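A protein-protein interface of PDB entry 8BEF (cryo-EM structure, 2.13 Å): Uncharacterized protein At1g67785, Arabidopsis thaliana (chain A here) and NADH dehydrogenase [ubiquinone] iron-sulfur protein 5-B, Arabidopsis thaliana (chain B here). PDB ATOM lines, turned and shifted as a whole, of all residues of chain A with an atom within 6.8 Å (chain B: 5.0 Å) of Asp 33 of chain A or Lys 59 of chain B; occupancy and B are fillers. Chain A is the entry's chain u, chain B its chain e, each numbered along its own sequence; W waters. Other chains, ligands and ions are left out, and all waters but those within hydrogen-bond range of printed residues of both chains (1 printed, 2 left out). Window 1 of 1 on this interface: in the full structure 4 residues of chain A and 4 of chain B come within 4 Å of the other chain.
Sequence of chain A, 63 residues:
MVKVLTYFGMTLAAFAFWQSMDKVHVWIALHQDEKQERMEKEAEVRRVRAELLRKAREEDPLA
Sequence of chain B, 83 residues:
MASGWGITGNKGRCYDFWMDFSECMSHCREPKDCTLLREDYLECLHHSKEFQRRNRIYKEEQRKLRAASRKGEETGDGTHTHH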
ATOM      1  N   ILE A  28       1.448   1.955  10.901  1.00  0.00           N
ATOM      2  CA  ILE A  28       1.073   0.928   9.930  1.00  0.00           C
ATOM      3  C   ILE A  28       0.450   1.565   8.695  1.00  0.00           C
ATOM      4  O   ILE A  28       0.743   1.169   7.560  1.00  0.00           O
ATOM      5  CB  ILE A  28       0.134  -0.109  10.572  1.00  0.00           C
ATOM      6  CG1 ILE A  28       0.910  -0.995  11.544  1.00  0.00           C
ATOM      7  CG2 ILE A  28      -0.524  -0.968   9.503  1.00  0.00           C
ATOM      8  CD1 ILE A  28       0.074  -1.537  12.665  1.00  0.00           C
ATOM      9  N   ALA A  29      -0.410   2.567   8.892  1.00  0.00           N
ATOM     10  CA  ALA A  29      -1.022   3.246   7.754  1.00  0.00           C
ATOM     11  C   ALA A  29       0.023   3.949   6.892  1.00  0.00           C
ATOM     12  O   ALA A  29      -0.064   3.924   5.658  1.00  0.00           O
ATOM     13  CB  ALA A  29      -2.073   4.245   8.237  1.00  0.00           C
ATOM     14  N   LEU A  30       1.020   4.578   7.519  1.00  0.00           N
ATOM     15  CA  LEU A  30       2.014   5.327   6.755  1.00  0.00           C
ATOM     16  C   LEU A  30       2.890   4.437   5.882  1.00  0.00           C
ATOM     17  O   LEU A  30       3.519   4.943   4.949  1.00  0.00           O
ATOM     18  CB  LEU A  30       2.897   6.153   7.691  1.00  0.00           C
ATOM     19  CG  LEU A  30       2.275   7.446   8.218  1.00  0.00           C
ATOM     20  CD1 LEU A  30       2.944   7.880   9.508  1.00  0.00           C
ATOM     21  CD2 LEU A  30       2.358   8.545   7.175  1.00  0.00           C
ATOM     22  N   HIS A  31       2.941   3.133   6.147  1.00  0.00           N
ATOM     23  CA  HIS A  31       3.800   2.220   5.406  1.00  0.00           C
ATOM     24  C   HIS A  31       3.035   1.352   4.414  1.00  0.00           C
ATOM     25  O   HIS A  31       3.560   0.325   3.973  1.00  0.00           O
ATOM     26  CB  HIS A  31       4.595   1.345   6.375  1.00  0.00           C
ATOM     27  CG  HIS A  31       5.731   2.065   7.031  1.00  0.00           C
ATOM     28  ND1 HIS A  31       5.545   3.017   8.009  1.00  0.00           N
ATOM     29  CD2 HIS A  31       7.069   1.979   6.838  1.00  0.00           C
ATOM     30  CE1 HIS A  31       6.719   3.486   8.393  1.00  0.00           C
ATOM     31  NE2 HIS A  31       7.661   2.871   7.699  1.00  0.00           N
ATOM     32  N   GLN A  32       1.808   1.737   4.057  1.00  0.00           N
ATOM     33  CA  GLN A  32       1.063   0.974   3.059  1.00  0.00           C
ATOM     34  C   GLN A  32       1.760   1.007   1.703  1.00  0.00           C
ATOM     35  O   GLN A  32       1.842  -0.016   1.014  1.00  0.00           O
ATOM     36  CB  GLN A  32      -0.363   1.512   2.938  1.00  0.00           C
ATOM     37  CG  GLN A  32      -1.306   1.076   4.046  1.00  0.00           C
ATOM     38  CD  GLN A  32      -1.248  -0.415   4.316  1.00  0.00           C
ATOM     39  OE1 GLN A  32      -0.673  -0.853   5.311  1.00  0.00           O
ATOM     40  NE2 GLN A  32      -1.846  -1.202   3.432  1.00  0.00           N
ATOM     41  N   ASP A  33       2.262   2.177   1.302  1.00  0.00           N
ATOM     42  CA  ASP A  33       2.850   2.320  -0.028  1.00  0.00           C
ATOM     43  C   ASP A  33       4.111   1.478  -0.184  1.00  0.00           C
ATOM     44  O   ASP A  33       4.297   0.819  -1.211  1.00  0.00           O
ATOM     45  CB  ASP A  33       3.149   3.789  -0.309  1.00  0.00           C
ATOM     46  CG  ASP A  33       2.083   4.715   0.241  1.00  0.00           C
ATOM     47  OD1 ASP A  33       1.049   4.904  -0.434  1.00  0.00           O
ATOM     48  OD2 ASP A  33       2.281   5.257   1.349  1.00  0.00           O
ATOM     49  N   GLU A  34       4.993   1.494   0.819  1.00  0.00           N
ATOM     50  CA  GLU A  34       6.209   0.688   0.742  1.00  0.00           C
ATOM     51  C   GLU A  34       5.885  -0.800   0.704  1.00  0.00           C
ATOM     52  O   GLU A  34       6.523  -1.563  -0.030  1.00  0.00           O
ATOM     53  CB  GLU A  34       7.131   1.002   1.919  1.00  0.00           C
ATOM     54  CG  GLU A  34       7.905   2.310   1.794  1.00  0.00           C
ATOM     55  CD  GLU A  34       7.007   3.533   1.790  1.00  0.00           C
ATOM     56  OE1 GLU A  34       6.708   4.059   2.881  1.00  0.00           O
ATOM     57  OE2 GLU A  34       6.605   3.969   0.691  1.00  0.00           O
ATOM     58  N   LYS A  35       4.906  -1.234   1.501  1.00  0.00           N
ATOM     59  CA  LYS A  35       4.499  -2.634   1.472  1.00  0.00           C
ATOM     60  C   LYS A  35       3.946  -3.012   0.105  1.00  0.00           C
ATOM     61  O   LYS A  35       4.232  -4.097  -0.412  1.00  0.00           O
ATOM     62  CB  LYS A  35       3.468  -2.907   2.566  1.00  0.00           C
ATOM     63  CG  LYS A  35       3.042  -4.357   2.665  1.00  0.00           C
ATOM     64  CD  LYS A  35       1.579  -4.478   3.063  1.00  0.00           C
ATOM     65  CE  LYS A  35       1.367  -4.073   4.511  1.00  0.00           C
ATOM     66  NZ  LYS A  35       0.866  -5.206   5.338  1.00  0.00           N
ATOM     67  N   GLN A  36       3.158  -2.121  -0.500  1.00  0.00           N
ATOM     68  CA  GLN A  36       2.661  -2.367  -1.849  1.00  0.00           C
ATOM     69  C   GLN A  36       3.807  -2.458  -2.849  1.00  0.00           C
ATOM     70  O   GLN A  36       3.793  -3.310  -3.742  1.00  0.00           O
ATOM     71  CB  GLN A  36       1.687  -1.267  -2.255  1.00  0.00           C
ATOM     72  CG  GLN A  36       0.235  -1.705  -2.307  1.00  0.00           C
ATOM     73  CD  GLN A  36      -0.610  -0.790  -3.167  1.00  0.00           C
ATOM     74  OE1 GLN A  36      -0.086   0.048  -3.901  1.00  0.00           O
ATOM     75  NE2 GLN A  36      -1.924  -0.946  -3.084  1.00  0.00           N
ATOM     76  N   GLU A  37       4.800  -1.579  -2.719  1.00  0.00           N
ATOM     77  CA  GLU A  37       5.947  -1.611  -3.621  1.00  0.00           C
ATOM     78  C   GLU A  37       6.716  -2.920  -3.488  1.00  0.00           C
ATOM     79  O   GLU A  37       7.120  -3.519  -4.491  1.00  0.00           O
ATOM     80  CB  GLU A  37       6.858  -0.418  -3.340  1.00  0.00           C
ATOM     81  CG  GLU A  37       8.004  -0.252  -4.322  1.00  0.00           C
ATOM     82  CD  GLU A  37       8.954   0.858  -3.918  1.00  0.00           C
ATOM     83  OE1 GLU A  37       8.763   1.434  -2.827  1.00  0.00           O
ATOM     84  OE2 GLU A  37       9.886   1.156  -4.693  1.00  0.00           O
ATOM     85  N   ARG A  38       6.927  -3.377  -2.251  1.00  0.00           N
ATOM     86  CA  ARG A  38       7.605  -4.650  -2.030  1.00  0.00           C
ATOM     87  C   ARG A  38       6.806  -5.806  -2.617  1.00  0.00           C
ATOM     88  O   ARG A  38       7.369  -6.702  -3.262  1.00  0.00           O
ATOM     89  CB  ARG A  38       7.837  -4.860  -0.535  1.00  0.00           C
ATOM     90  CG  ARG A  38       8.995  -5.782  -0.198  1.00  0.00           C
ATOM     91  CD  ARG A  38       8.639  -6.715   0.949  1.00  0.00           C
ATOM     92  NE  ARG A  38       7.837  -6.054   1.974  1.00  0.00           N
ATOM     93  CZ  ARG A  38       8.321  -5.225   2.889  1.00  0.00           C
ATOM     94  NH1 ARG A  38       9.610  -4.925   2.938  1.00  0.00           N
ATOM     95  NH2 ARG A  38       7.494  -4.685   3.778  1.00  0.00           N
ATOM     96  N   GLN B  52      -6.048   5.101   1.133  1.00  0.00           N
ATOM     97  CA  GLN B  52      -4.634   4.993   0.786  1.00  0.00           C
ATOM     98  C   GLN B  52      -4.178   6.183  -0.055  1.00  0.00           C
ATOM     99  O   GLN B  52      -3.110   6.759   0.191  1.00  0.00           O
ATOM    100  CB  GLN B  52      -4.380   3.687   0.039  1.00  0.00           C
ATOM    101  CG  GLN B  52      -2.921   3.421  -0.263  1.00  0.00           C
ATOM    102  CD  GLN B  52      -2.569   1.956  -0.141  1.00  0.00           C
ATOM    103  OE1 GLN B  52      -3.432   1.115   0.101  1.00  0.00           O
ATOM    104  NE2 GLN B  52      -1.290   1.646  -0.291  1.00  0.00           N
ATOM    105  N   ASN B  55      -4.018   9.261   2.044  1.00  0.00           N
ATOM    106  CA  ASN B  55      -2.836   9.203   2.892  1.00  0.00           C
ATOM    107  C   ASN B  55      -1.574   9.516   2.105  1.00  0.00           C
ATOM    108  O   ASN B  55      -0.640  10.098   2.654  1.00  0.00           O
ATOM    109  CB  ASN B  55      -2.725   7.833   3.554  1.00  0.00           C
ATOM    110  CG  ASN B  55      -3.786   7.613   4.618  1.00  0.00           C
ATOM    111  OD1 ASN B  55      -4.445   8.555   5.056  1.00  0.00           O
ATOM    112  ND2 ASN B  55      -3.952   6.368   5.040  1.00  0.00           N
ATOM    113  N   ARG B  56      -1.524   9.129   0.829  1.00  0.00           N
ATOM    114  CA  ARG B  56      -0.417   9.557  -0.022  1.00  0.00           C
ATOM    115  C   ARG B  56      -0.368  11.076  -0.129  1.00  0.00           C
ATOM    116  O   ARG B  56       0.712  11.680  -0.078  1.00  0.00           O
ATOM    117  CB  ARG B  56      -0.542   8.930  -1.410  1.00  0.00           C
ATOM    118  CG  ARG B  56       0.417   7.797  -1.656  1.00  0.00           C
ATOM    119  CD  ARG B  56       0.227   7.191  -3.025  1.00  0.00           C
ATOM    120  NE  ARG B  56       0.025   5.749  -2.960  1.00  0.00           N
ATOM    121  CZ  ARG B  56      -1.151   5.153  -3.082  1.00  0.00           C
ATOM    122  NH1 ARG B  56      -2.257   5.846  -3.294  1.00  0.00           N
ATOM    123  NH2 ARG B  56      -1.219   3.828  -2.997  1.00  0.00           N
ATOM    124  N   ILE B  57      -1.532  11.709  -0.279  1.00  0.00           N
ATOM    125  CA  ILE B  57      -1.571  13.170  -0.347  1.00  0.00           C
ATOM    126  C   ILE B  57      -1.045  13.776   0.951  1.00  0.00           C
ATOM    127  O   ILE B  57      -0.227  14.707   0.943  1.00  0.00           O
ATOM    128  CB  ILE B  57      -2.995  13.661  -0.662  1.00  0.00           C
ATOM    129  CG1 ILE B  57      -3.350  13.373  -2.119  1.00  0.00           C
ATOM    130  CG2 ILE B  57      -3.128  15.153  -0.373  1.00  0.00           C
ATOM    131  CD1 ILE B  57      -4.833  13.335  -2.375  1.00  0.00           C
ATOM    132  N   TYR B  58      -1.503  13.245   2.086  1.00  0.00           N
ATOM    133  CA  TYR B  58      -1.030  13.729   3.383  1.00  0.00           C
ATOM    134  C   TYR B  58       0.472  13.510   3.546  1.00  0.00           C
ATOM    135  O   TYR B  58       1.179  14.357   4.107  1.00  0.00           O
ATOM    136  CB  TYR B  58      -1.807  13.040   4.505  1.00  0.00           C
ATOM    137  CG  TYR B  58      -1.106  13.017   5.847  1.00  0.00           C
ATOM    138  CD1 TYR B  58      -1.167  14.106   6.705  1.00  0.00           C
ATOM    139  CD2 TYR B  58      -0.390  11.901   6.257  1.00  0.00           C
ATOM    140  CE1 TYR B  58      -0.531  14.084   7.930  1.00  0.00           C
ATOM    141  CE2 TYR B  58       0.250  11.873   7.480  1.00  0.00           C
ATOM    142  CZ  TYR B  58       0.176  12.962   8.311  1.00  0.00           C
ATOM    143  OH  TYR B  58       0.814  12.931   9.529  1.00  0.00           O
ATOM    144  N   LYS B  59       0.971  12.370   3.067  1.00  0.00           N
ATOM    145  CA  LYS B  59       2.395  12.061   3.130  1.00  0.00           C
ATOM    146  C   LYS B  59       3.210  13.083   2.353  1.00  0.00           C
ATOM    147  O   LYS B  59       4.229  13.584   2.840  1.00  0.00           O
ATOM    148  CB  LYS B  59       2.637  10.661   2.571  1.00  0.00           C
ATOM    149  CG  LYS B  59       3.944  10.021   2.974  1.00  0.00           C
ATOM    150  CD  LYS B  59       3.820   8.505   2.993  1.00  0.00           C
ATOM    151  CE  LYS B  59       2.419   8.058   3.380  1.00  0.00           C
ATOM    152  NZ  LYS B  59       2.372   6.602   3.672  1.00  0.00           N
ATOM    153  N   GLU B  60       2.783  13.388   1.128  1.00  0.00           N
ATOM    154  CA  GLU B  60       3.505  14.369   0.325  1.00  0.00           C
ATOM    155  C   GLU B  60       3.448  15.750   0.967  1.00  0.00           C
ATOM    156  O   GLU B  60       4.423  16.511   0.915  1.00  0.00           O
ATOM    157  CB  GLU B  60       2.943  14.401  -1.095  1.00  0.00           C
ATOM    158  CG  GLU B  60       3.662  15.369  -2.015  1.00  0.00           C
ATOM    159  CD  GLU B  60       4.947  14.788  -2.570  1.00  0.00           C
ATOM    160  OE1 GLU B  60       4.974  13.576  -2.871  1.00  0.00           O
ATOM    161  OE2 GLU B  60       5.931  15.544  -2.705  1.00  0.00           O
ATOM    162  N   GLU B  61       2.317  16.085   1.593  1.00  0.00           N
ATOM    163  CA  GLU B  61       2.237  17.350   2.317  1.00  0.00           C
ATOM    164  C   GLU B  61       3.235  17.391   3.467  1.00  0.00           C
ATOM    165  O   GLU B  61       3.887  18.416   3.696  1.00  0.00           O
ATOM    166  CB  GLU B  61       0.818  17.578   2.836  1.00  0.00           C
ATOM    167  CG  GLU B  61       0.503  19.032   3.114  1.00  0.00           C
ATOM    168  CD  GLU B  61      -0.729  19.209   3.979  1.00  0.00           C
ATOM    169  OE1 GLU B  61      -1.146  18.230   4.632  1.00  0.00           O
ATOM    170  OE2 GLU B  61      -1.279  20.329   4.007  1.00  0.00           O
ATOM    171  N   GLN B  62       3.370  16.287   4.202  1.00  0.00           N
ATOM    172  CA  GLN B  62       4.321  16.258   5.309  1.00  0.00           C
ATOM    173  C   GLN B  62       5.762  16.257   4.812  1.00  0.00           C
ATOM    174  O   GLN B  62       6.663  16.723   5.517  1.00  0.00           O
ATOM    175  CB  GLN B  62       4.065  15.040   6.196  1.00  0.00           C
ATOM    176  CG  GLN B  62       4.001  15.335   7.689  1.00  0.00           C
ATOM    177  CD  GLN B  62       2.925  16.346   8.054  1.00  0.00           C
ATOM    178  OE1 GLN B  62       1.948  16.526   7.327  1.00  0.00           O
ATOM    179  NE2 GLN B  62       3.103  17.011   9.188  1.00  0.00           N
ATOM    180  N   ARG B  63       5.997  15.726   3.611  1.00  0.00           N
ATOM    181  CA  ARG B  63       7.344  15.710   3.054  1.00  0.00           C
ATOM    182  C   ARG B  63       7.763  17.094   2.567  1.00  0.00           C
ATOM    183  O   ARG B  63       8.922  17.490   2.735  1.00  0.00           O
ATOM    184  CB  ARG B  63       7.426  14.693   1.917  1.00  0.00           C
ATOM    185  CG  ARG B  63       8.825  14.424   1.427  1.00  0.00           C
ATOM    186  CD  ARG B  63       8.811  13.732   0.076  1.00  0.00           C
ATOM    187  NE  ARG B  63       8.287  14.588  -0.979  1.00  0.00           N
ATOM    188  CZ  ARG B  63       8.994  15.512  -1.614  1.00  0.00           C
ATOM    189  NH1 ARG B  63      10.262  15.741  -1.311  1.00  0.00           N
ATOM    190  NH2 ARG B  63       8.417  16.222  -2.578  1.00  0.00           N
HETATM  191  O   HOH W   1      -2.116   4.503   3.809  1.00  0.00           O
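The side-chain carboxylate (OD2) of Asp 33 of chain A lies within salt-bridge range of the side-chain amino group (NZ) of Lys 59 of chain B, at 2.7 Å. NE of Arg 56 of chain B lies within salt-bridge range of OD1 of Asp 33 of chain A, 2.9 Å away. The backbone carbonyl oxygen (O) of Leu 30 of chain A sits close to the side-chain amino group (NZ) of Lys 59 of chain B (2.4 Å).
NE2 of Gln 52 of chain B lies close to NH2 of Arg 56 of chain B (3.5 Å). O of Ile 28 of chain A lies close to OE1 of Gln 32 of chain A (3.3 Å).
Tyr 58 of chain B touches Leu 30 of chain A. NE2 of Gln 52 of chain B touches CB of Gln 32 of chain A, at 3.4 Å. Asp 33 of chain A touches Gln 52 of chain B. Gln 52 of chain B touches Gln 36 of chain A.
Asp 33 of chain A touches just these residues of chain B: Gln 52 (3.9 Å), Arg 56 (2.9 Å) and Lys 59 (2.7 Å). Of the printed residues of chain B, Gln 36 of chain A touches Gln 52. Of the printed residues of chain A, Gln 52 of chain B touches Gln 32, Asp 33 and Gln 36. Of the printed residues of chain A, Arg 56 of chain B touches Asp 33 (2.9 Å). Lys 59 of chain B touches just these residues of chain A: Leu 30 (2.4 Å) and Asp 33 (2.7 Å). The nearest residue of chain A that does not touch Lys 59 of chain B is Ala 29 of chain A (4.1 Å). The nearest printed residue of chain A that does not touch Tyr 58 of chain B is Ala 29 of chain A (7.9 Å).
Printed residues of chain A that touch a printed residue of chain B: Leu 30, Gln 32, Asp 33 and Gln 36. Of the 10 printed residues of chain B, 4 touch a printed residue of chain A. Hydrophobic or aromatic side chains of chain B within 4 Å of the printed part of chain A: Tyr 58. Among the printed residues, 7 pairs touch across the chains. Among the printed residues, Asp or Glu carboxylates within 4 Å of a Lys or Arg side-chain nitrogen of the other chain: Asp 33 of chain A with Arg 56 of chain B (2.9 Å) and Asp 33 of chain A with Lys 59 of chain B (2.7 Å).
Water W1 bridges the backbone carbonyl oxygen of Ala 29 of chain A and the side-chain amide nitrogen of Asn 55 of chain B.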
